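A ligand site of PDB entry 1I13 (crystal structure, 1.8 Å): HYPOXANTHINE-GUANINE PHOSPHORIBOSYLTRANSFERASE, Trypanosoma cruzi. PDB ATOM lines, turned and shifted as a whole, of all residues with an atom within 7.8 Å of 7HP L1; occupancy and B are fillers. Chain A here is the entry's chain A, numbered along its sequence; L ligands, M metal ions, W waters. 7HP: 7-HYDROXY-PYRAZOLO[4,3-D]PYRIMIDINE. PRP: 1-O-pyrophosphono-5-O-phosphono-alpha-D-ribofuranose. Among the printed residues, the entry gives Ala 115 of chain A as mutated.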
ATOM      1  N   ASP A 112     -20.511  23.638  25.449  1.00  0.00           N
ATOM      2  CA  ASP A 112     -19.210  23.335  24.895  1.00  0.00           C
ATOM      3  C   ASP A 112     -18.824  24.348  23.819  1.00  0.00           C
ATOM      4  O   ASP A 112     -17.690  24.850  23.797  1.00  0.00           O
ATOM      5  CB  ASP A 112     -19.212  21.907  24.299  1.00  0.00           C
ATOM      6  CG  ASP A 112     -20.407  21.657  23.356  1.00  0.00           C
ATOM      7  OD1 ASP A 112     -21.332  22.506  23.257  1.00  0.00           O
ATOM      8  OD2 ASP A 112     -20.437  20.580  22.724  1.00  0.00           O
ATOM      9  N   ILE A 113     -19.783  24.712  22.983  1.00  0.00           N
ATOM     10  CA  ILE A 113     -19.509  25.648  21.909  1.00  0.00           C
ATOM     11  C   ILE A 113     -20.708  26.490  21.522  1.00  0.00           C
ATOM     12  O   ILE A 113     -21.866  26.041  21.570  1.00  0.00           O
ATOM     13  CB  ILE A 113     -19.009  24.873  20.660  1.00  0.00           C
ATOM     14  CG1 ILE A 113     -18.389  25.834  19.639  1.00  0.00           C
ATOM     15  CG2 ILE A 113     -20.149  24.091  20.022  1.00  0.00           C
ATOM     16  CD1 ILE A 113     -17.570  25.145  18.572  1.00  0.00           C
ATOM     17  N   VAL A 114     -20.425  27.749  21.187  1.00  0.00           N
ATOM     18  CA  VAL A 114     -21.449  28.661  20.696  1.00  0.00           C
ATOM     19  C   VAL A 114     -20.937  29.215  19.365  1.00  0.00           C
ATOM     20  O   VAL A 114     -19.751  29.483  19.211  1.00  0.00           O
ATOM     21  CB  VAL A 114     -21.794  29.749  21.722  1.00  0.00           C
ATOM     22  CG1 VAL A 114     -20.619  30.673  21.955  1.00  0.00           C
ATOM     23  CG2 VAL A 114     -23.058  30.481  21.283  1.00  0.00           C
ATOM     24  N   ALA A 115     -21.787  29.166  18.354  1.00  0.00           N
ATOM     25  CA  ALA A 115     -21.457  29.653  17.021  1.00  0.00           C
ATOM     26  C   ALA A 115     -22.631  30.509  16.546  1.00  0.00           C
ATOM     27  O   ALA A 115     -22.602  31.732  16.691  1.00  0.00           O
ATOM     28  CB  ALA A 115     -21.216  28.487  16.070  1.00  0.00           C
ATOM     29  N   THR A 116     -23.677  29.852  16.029  1.00  0.00           N
ATOM     30  CA  THR A 116     -24.859  30.584  15.559  1.00  0.00           C
ATOM     31  C   THR A 116     -25.584  31.186  16.743  1.00  0.00           C
ATOM     32  O   THR A 116     -26.204  32.255  16.622  1.00  0.00           O
ATOM     33  CB  THR A 116     -25.840  29.676  14.748  1.00  0.00           C
ATOM     34  OG1 THR A 116     -26.579  28.834  15.642  1.00  0.00           O
ATOM     35  CG2 THR A 116     -25.077  28.823  13.738  1.00  0.00           C
ATOM     36  N   LEU A 141     -15.858  26.960  24.007  1.00  0.00           N
ATOM     37  CA  LEU A 141     -15.395  27.543  22.750  1.00  0.00           C
ATOM     38  C   LEU A 141     -16.394  28.539  22.163  1.00  0.00           C
ATOM     39  O   LEU A 141     -17.598  28.348  22.284  1.00  0.00           O
ATOM     40  CB  LEU A 141     -15.161  26.449  21.717  1.00  0.00           C
ATOM     41  CG  LEU A 141     -14.171  25.337  22.077  1.00  0.00           C
ATOM     42  CD1 LEU A 141     -14.142  24.404  20.906  1.00  0.00           C
ATOM     43  CD2 LEU A 141     -12.769  25.880  22.344  1.00  0.00           C
ATOM     44  N   LYS A 143     -17.183  30.645  18.510  1.00  0.00           N
ATOM     45  CA  LYS A 143     -16.885  31.040  17.131  1.00  0.00           C
ATOM     46  C   LYS A 143     -17.608  32.382  17.026  1.00  0.00           C
ATOM     47  O   LYS A 143     -18.754  32.455  16.585  1.00  0.00           O
ATOM     48  CB  LYS A 143     -17.493  30.074  16.127  1.00  0.00           C
ATOM     49  CG  LYS A 143     -16.798  28.759  16.016  1.00  0.00           C
ATOM     50  CD  LYS A 143     -17.510  27.905  14.981  1.00  0.00           C
ATOM     51  CE  LYS A 143     -16.962  26.507  14.977  1.00  0.00           C
ATOM     52  NZ  LYS A 143     -17.876  25.595  14.261  1.00  0.00           N
ATOM     53  N   ILE A 160     -12.483  30.810  18.901  1.00  0.00           N
ATOM     54  CA  ILE A 160     -11.843  30.010  17.866  1.00  0.00           C
ATOM     55  C   ILE A 160     -12.329  30.439  16.511  1.00  0.00           C
ATOM     56  O   ILE A 160     -13.339  31.119  16.397  1.00  0.00           O
ATOM     57  CB  ILE A 160     -12.170  28.476  18.018  1.00  0.00           C
ATOM     58  CG1 ILE A 160     -13.670  28.267  18.135  1.00  0.00           C
ATOM     59  CG2 ILE A 160     -11.495  27.916  19.232  1.00  0.00           C
ATOM     60  CD1 ILE A 160     -14.113  26.867  17.845  1.00  0.00           C
ATOM     61  N   PRO A 161     -11.586  30.067  15.449  1.00  0.00           N
ATOM     62  CA  PRO A 161     -11.933  30.404  14.068  1.00  0.00           C
ATOM     63  C   PRO A 161     -13.129  29.568  13.654  1.00  0.00           C
ATOM     64  O   PRO A 161     -13.530  28.645  14.372  1.00  0.00           O
ATOM     65  CB  PRO A 161     -10.696  29.951  13.286  1.00  0.00           C
ATOM     66  CG  PRO A 161      -9.600  29.885  14.318  1.00  0.00           C
ATOM     67  CD  PRO A 161     -10.309  29.330  15.505  1.00  0.00           C
ATOM     68  N   ASN A 162     -13.644  29.838  12.468  1.00  0.00           N
ATOM     69  CA  ASN A 162     -14.781  29.113  11.960  1.00  0.00           C
ATOM     70  C   ASN A 162     -14.349  27.857  11.241  1.00  0.00           C
ATOM     71  O   ASN A 162     -14.227  27.838  10.010  1.00  0.00           O
ATOM     72  CB  ASN A 162     -15.603  29.981  11.014  1.00  0.00           C
ATOM     73  CG  ASN A 162     -16.992  30.225  11.533  1.00  0.00           C
ATOM     74  OD1 ASN A 162     -17.274  31.286  12.087  1.00  0.00           O
ATOM     75  ND2 ASN A 162     -17.867  29.237  11.388  1.00  0.00           N
ATOM     76  N   ALA A 163     -14.049  26.830  12.007  1.00  0.00           N
ATOM     77  CA  ALA A 163     -13.648  25.546  11.473  1.00  0.00           C
ATOM     78  C   ALA A 163     -14.388  24.560  12.376  1.00  0.00           C
ATOM     79  O   ALA A 163     -14.736  24.893  13.520  1.00  0.00           O
ATOM     80  CB  ALA A 163     -12.151  25.378  11.617  1.00  0.00           C
ATOM     81  N   PHE A 164     -14.692  23.369  11.861  1.00  0.00           N
ATOM     82  CA  PHE A 164     -15.398  22.389  12.658  1.00  0.00           C
ATOM     83  C   PHE A 164     -14.408  21.703  13.595  1.00  0.00           C
ATOM     84  O   PHE A 164     -13.437  21.099  13.137  1.00  0.00           O
ATOM     85  CB  PHE A 164     -16.089  21.362  11.766  1.00  0.00           C
ATOM     86  CG  PHE A 164     -17.192  20.616  12.468  1.00  0.00           C
ATOM     87  CD1 PHE A 164     -18.428  21.207  12.661  1.00  0.00           C
ATOM     88  CD2 PHE A 164     -16.990  19.325  12.955  1.00  0.00           C
ATOM     89  CE1 PHE A 164     -19.449  20.537  13.342  1.00  0.00           C
ATOM     90  CE2 PHE A 164     -18.001  18.651  13.627  1.00  0.00           C
ATOM     91  CZ  PHE A 164     -19.234  19.261  13.814  1.00  0.00           C
ATOM     92  N   VAL A 165     -14.621  21.882  14.896  1.00  0.00           N
ATOM     93  CA  VAL A 165     -13.762  21.292  15.920  1.00  0.00           C
ATOM     94  C   VAL A 165     -14.400  20.023  16.508  1.00  0.00           C
ATOM     95  O   VAL A 165     -15.622  19.899  16.558  1.00  0.00           O
ATOM     96  CB  VAL A 165     -13.457  22.297  17.080  1.00  0.00           C
ATOM     97  CG1 VAL A 165     -12.543  23.404  16.588  1.00  0.00           C
ATOM     98  CG2 VAL A 165     -14.724  22.907  17.621  1.00  0.00           C
ATOM     99  N   ILE A 166     -13.568  19.101  16.971  1.00  0.00           N
ATOM    100  CA  ILE A 166     -14.031  17.858  17.562  1.00  0.00           C
ATOM    101  C   ILE A 166     -13.160  17.539  18.769  1.00  0.00           C
ATOM    102  O   ILE A 166     -12.063  18.105  18.917  1.00  0.00           O
ATOM    103  CB  ILE A 166     -13.923  16.668  16.566  1.00  0.00           C
ATOM    104  CG1 ILE A 166     -12.577  16.709  15.842  1.00  0.00           C
ATOM    105  CG2 ILE A 166     -15.088  16.687  15.589  1.00  0.00           C
ATOM    106  CD1 ILE A 166     -12.347  15.540  14.913  1.00  0.00           C
ATOM    107  N   GLY A 167     -13.634  16.633  19.618  1.00  0.00           N
ATOM    108  CA  GLY A 167     -12.871  16.258  20.790  1.00  0.00           C
ATOM    109  C   GLY A 167     -13.357  16.981  22.012  1.00  0.00           C
ATOM    110  O   GLY A 167     -14.113  17.956  21.928  1.00  0.00           O
ATOM    111  N   GLY A 169     -15.592  16.300  24.114  1.00  0.00           N
ATOM    112  CA  GLY A 169     -17.043  16.354  24.188  1.00  0.00           C
ATOM    113  C   GLY A 169     -17.685  16.688  22.861  1.00  0.00           C
ATOM    114  O   GLY A 169     -18.818  16.267  22.611  1.00  0.00           O
ATOM    115  N   LEU A 170     -16.968  17.388  22.007  1.00  0.00           N
ATOM    116  CA  LEU A 170     -17.469  17.787  20.692  1.00  0.00           C
ATOM    117  C   LEU A 170     -17.363  16.659  19.689  1.00  0.00           C
ATOM    118  O   LEU A 170     -16.329  16.016  19.575  1.00  0.00           O
ATOM    119  CB  LEU A 170     -16.683  18.976  20.157  1.00  0.00           C
ATOM    120  CG  LEU A 170     -16.744  20.243  21.006  1.00  0.00           C
ATOM    121  CD1 LEU A 170     -15.592  21.127  20.597  1.00  0.00           C
ATOM    122  CD2 LEU A 170     -18.073  20.932  20.787  1.00  0.00           C
ATOM    123  N   ASP A 171     -18.405  16.455  18.920  1.00  0.00           N
ATOM    124  CA  ASP A 171     -18.407  15.359  17.971  1.00  0.00           C
ATOM    125  C   ASP A 171     -18.675  15.746  16.555  1.00  0.00           C
ATOM    126  O   ASP A 171     -19.089  16.866  16.242  1.00  0.00           O
ATOM    127  CB  ASP A 171     -19.567  14.405  18.317  1.00  0.00           C
ATOM    128  CG  ASP A 171     -20.943  15.031  18.033  1.00  0.00           C
ATOM    129  OD1 ASP A 171     -21.268  16.089  18.630  1.00  0.00           O
ATOM    130  OD2 ASP A 171     -21.714  14.461  17.231  1.00  0.00           O
ATOM    131  N   TYR A 172     -18.516  14.740  15.715  1.00  0.00           N
ATOM    132  CA  TYR A 172     -18.898  14.826  14.321  1.00  0.00           C
ATOM    133  C   TYR A 172     -19.570  13.473  14.112  1.00  0.00           C
ATOM    134  O   TYR A 172     -18.906  12.432  14.246  1.00  0.00           O
ATOM    135  CB  TYR A 172     -17.745  14.939  13.339  1.00  0.00           C
ATOM    136  CG  TYR A 172     -18.289  14.674  11.952  1.00  0.00           C
ATOM    137  CD1 TYR A 172     -19.439  15.352  11.496  1.00  0.00           C
ATOM    138  CD2 TYR A 172     -17.770  13.655  11.155  1.00  0.00           C
ATOM    139  CE1 TYR A 172     -20.052  15.007  10.308  1.00  0.00           C
ATOM    140  CE2 TYR A 172     -18.373  13.306   9.958  1.00  0.00           C
ATOM    141  CZ  TYR A 172     -19.514  13.984   9.544  1.00  0.00           C
ATOM    142  OH  TYR A 172     -20.118  13.637   8.356  1.00  0.00           O
ATOM    143  N   ARG A 177     -15.963  12.392  20.519  1.00  0.00           N
ATOM    144  CA  ARG A 177     -16.215  13.189  21.719  1.00  0.00           C
ATOM    145  C   ARG A 177     -15.227  12.812  22.818  1.00  0.00           C
ATOM    146  O   ARG A 177     -14.961  13.621  23.711  1.00  0.00           O
ATOM    147  CB  ARG A 177     -17.617  12.937  22.295  1.00  0.00           C
ATOM    148  CG  ARG A 177     -18.824  13.099  21.392  1.00  0.00           C
ATOM    149  CD  ARG A 177     -20.062  13.147  22.267  1.00  0.00           C
ATOM    150  NE  ARG A 177     -21.297  13.156  21.512  1.00  0.00           N
ATOM    151  CZ  ARG A 177     -21.913  14.258  21.101  1.00  0.00           C
ATOM    152  NH1 ARG A 177     -21.397  15.456  21.385  1.00  0.00           N
ATOM    153  NH2 ARG A 177     -23.004  14.149  20.378  1.00  0.00           N
ATOM    154  N   ILE A 182      -8.730  19.133  21.699  1.00  0.00           N
ATOM    155  CA  ILE A 182      -9.660  19.744  20.752  1.00  0.00           C
ATOM    156  C   ILE A 182      -8.880  19.920  19.453  1.00  0.00           C
ATOM    157  O   ILE A 182      -7.844  20.581  19.418  1.00  0.00           O
ATOM    158  CB  ILE A 182     -10.219  21.113  21.242  1.00  0.00           C
ATOM    159  CG1 ILE A 182     -10.950  20.926  22.565  1.00  0.00           C
ATOM    160  CG2 ILE A 182     -11.215  21.664  20.230  1.00  0.00           C
ATOM    161  CD1 ILE A 182     -11.062  22.188  23.406  1.00  0.00           C
ATOM    162  N   VAL A 183      -9.386  19.303  18.403  1.00  0.00           N
ATOM    163  CA  VAL A 183      -8.716  19.353  17.118  1.00  0.00           C
ATOM    164  C   VAL A 183      -9.693  19.805  16.029  1.00  0.00           C
ATOM    165  O   VAL A 183     -10.908  19.845  16.252  1.00  0.00           O
ATOM    166  CB  VAL A 183      -8.098  17.930  16.768  1.00  0.00           C
ATOM    167  CG1 VAL A 183      -7.302  17.364  17.952  1.00  0.00           C
ATOM    168  CG2 VAL A 183      -9.184  16.945  16.333  1.00  0.00           C
ATOM    169  N   VAL A 184      -9.158  20.222  14.892  1.00  0.00           N
ATOM    170  CA  VAL A 184      -9.988  20.635  13.782  1.00  0.00           C
ATOM    171  C   VAL A 184     -10.115  19.447  12.850  1.00  0.00           C
ATOM    172  O   VAL A 184      -9.100  18.820  12.481  1.00  0.00           O
ATOM    173  CB  VAL A 184      -9.378  21.801  12.995  1.00  0.00           C
ATOM    174  CG1 VAL A 184     -10.238  22.130  11.795  1.00  0.00           C
ATOM    175  CG2 VAL A 184      -9.237  23.008  13.891  1.00  0.00           C
ATOM    176  N   LEU A 185     -11.340  19.131  12.476  1.00  0.00           N
ATOM    177  CA  LEU A 185     -11.622  18.003  11.600  1.00  0.00           C
ATOM    178  C   LEU A 185     -11.231  18.327  10.167  1.00  0.00           C
ATOM    179  O   LEU A 185     -11.542  19.413   9.676  1.00  0.00           O
ATOM    180  CB  LEU A 185     -13.117  17.674  11.668  1.00  0.00           C
ATOM    181  CG  LEU A 185     -13.659  16.455  10.922  1.00  0.00           C
ATOM    182  CD1 LEU A 185     -13.045  15.176  11.487  1.00  0.00           C
ATOM    183  CD2 LEU A 185     -15.164  16.431  11.060  1.00  0.00           C
HETATM  184  C9  7HP L   1     -21.526  22.992  16.525  1.00  0.00           C
HETATM  185  C4  7HP L   1     -20.360  22.241  16.544  1.00  0.00           C
HETATM  186  N3  7HP L   1     -20.202  21.006  17.057  1.00  0.00           N
HETATM  187  C2  7HP L   1     -18.891  20.605  16.946  1.00  0.00           C
HETATM  188  N1  7HP L   1     -17.901  21.373  16.372  1.00  0.00           N
HETATM  189  C6  7HP L   1     -18.086  22.626  15.834  1.00  0.00           C
HETATM  190  O6  7HP L   1     -17.176  23.190  15.277  1.00  0.00           O
HETATM  191  C5  7HP L   1     -19.387  23.028  15.955  1.00  0.00           C
HETATM  192  N7  7HP L   1     -19.982  24.215  15.593  1.00  0.00           N
HETATM  193  N8  7HP L   1     -21.221  24.126  15.945  1.00  0.00           N
HETATM  194  C1  PRP L   2     -23.779  21.334  19.141  1.00  0.00           C
HETATM  195  C2  PRP L   2     -22.976  21.990  20.230  1.00  0.00           C
HETATM  196  C3  PRP L   2     -24.032  23.052  20.664  1.00  0.00           C
HETATM  197  C4  PRP L   2     -24.597  23.418  19.306  1.00  0.00           C
HETATM  198  C5  PRP L   2     -23.874  24.681  18.855  1.00  0.00           C
HETATM  199  O1  PRP L   2     -24.772  20.503  19.825  1.00  0.00           O
HETATM  200  O2  PRP L   2     -22.622  20.875  21.124  1.00  0.00           O
HETATM  201  O3  PRP L   2     -25.187  22.497  21.344  1.00  0.00           O
HETATM  202  O4  PRP L   2     -24.431  22.292  18.344  1.00  0.00           O
HETATM  203  O5  PRP L   2     -24.121  24.931  17.445  1.00  0.00           O
HETATM  204  P   PRP L   2     -24.464  26.387  16.757  1.00  0.00           P
HETATM  205  O1P PRP L   2     -24.180  27.374  17.881  1.00  0.00           O
HETATM  206  O2P PRP L   2     -25.902  26.284  16.429  1.00  0.00           O
HETATM  207  O3P PRP L   2     -23.612  26.301  15.500  1.00  0.00           O
HETATM  208  PA  PRP L   2     -25.382  19.268  18.949  1.00  0.00           P
HETATM  209  O1A PRP L   2     -26.574  19.727  18.212  1.00  0.00           O
HETATM  210  O2A PRP L   2     -24.264  18.953  18.067  1.00  0.00           O
HETATM  211  O3A PRP L   2     -25.677  18.339  20.074  1.00  0.00           O
HETATM  212  PB  PRP L   2     -24.660  17.598  20.870  1.00  0.00           P
HETATM  213  O1B PRP L   2     -23.582  17.125  19.928  1.00  0.00           O
HETATM  214  O2B PRP L   2     -25.356  16.506  21.533  1.00  0.00           O
HETATM  215  O3B PRP L   2     -24.088  18.403  21.950  1.00  0.00           O
HETATM  216 MG    MG M   1     -22.713  17.507  18.103  1.00  0.00          MG
HETATM  217 MG    MG M   2     -24.488  20.588  22.407  1.00  0.00          MG
HETATM  218  O   HOH W   1     -21.466  18.926  18.862  1.00  0.00           O
HETATM  219  O   HOH W   2     -19.852  26.425  12.925  1.00  0.00           O
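NZ of Lys 143 sits at hydrogen-bond distance from O6 of 7HP L1, 2.7 Å away.
The backbone carbonyl oxygen of Ala 163 sits at hydrogen-bond distance from an oxygen (O6) of 7HP L1 (3.5 Å).
OD2 of Asp 112 lies close to O2 of PRP L2 (2.7 Å).
N of Thr 116 lies within hydrogen-bond range of O1P of PRP L2 (3.1 Å).
N of Val 165 is in hydrogen-bond range of O6 of 7HP L1.
An oxygen (O1P) of PRP L2 lies within hydrogen-bond range of the backbone NH (N) of Ala 115, at 3.0 Å.
O of Val 165 sits close to N1 of 7HP L1 (2.7 Å).
The guanidinium group (NH2) of Arg 177 is in salt-bridge range of an oxygen (O2B) of PRP L2 (3.5 Å).
The side-chain hydroxyl of Thr 116 is in hydrogen-bond range of an oxygen (O2P) of PRP L2, at 2.8 Å.
A nitrogen (N8) of 7HP L1 sits close to an oxygen (O3P) of PRP L2 (3.3 Å).
The guanidinium group (NH2) of Arg 177 is in salt-bridge range of the side-chain carboxylate (OD2) of Asp 171.
The backbone NH (N) of Lys 143 sits at hydrogen-bond distance from the backbone carbonyl oxygen (O) of Val 114, 2.9 Å away.
NZ of Lys 143 sits close to O of Ala 163 (3.3 Å).
The backbone NH of Leu 185 lies within hydrogen-bond range of the backbone carbonyl oxygen of Phe 164 (3.0 Å).
Ile 113 touches 7HP L1 (CD1 to C6, 3.8 Å).
Phe 164 touches 7HP L1.
Leu 170 touches 7HP L1.
Asp 171 touches 7HP L1 (O to C2, 3.8 Å).
Hydrophobic or aromatic side chains that line 7HP L1: Ile 113, Phe 164, Val 165 and Leu 170.
Water W2 bridges NZ of Lys 143 and N7 of 7HP L1.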
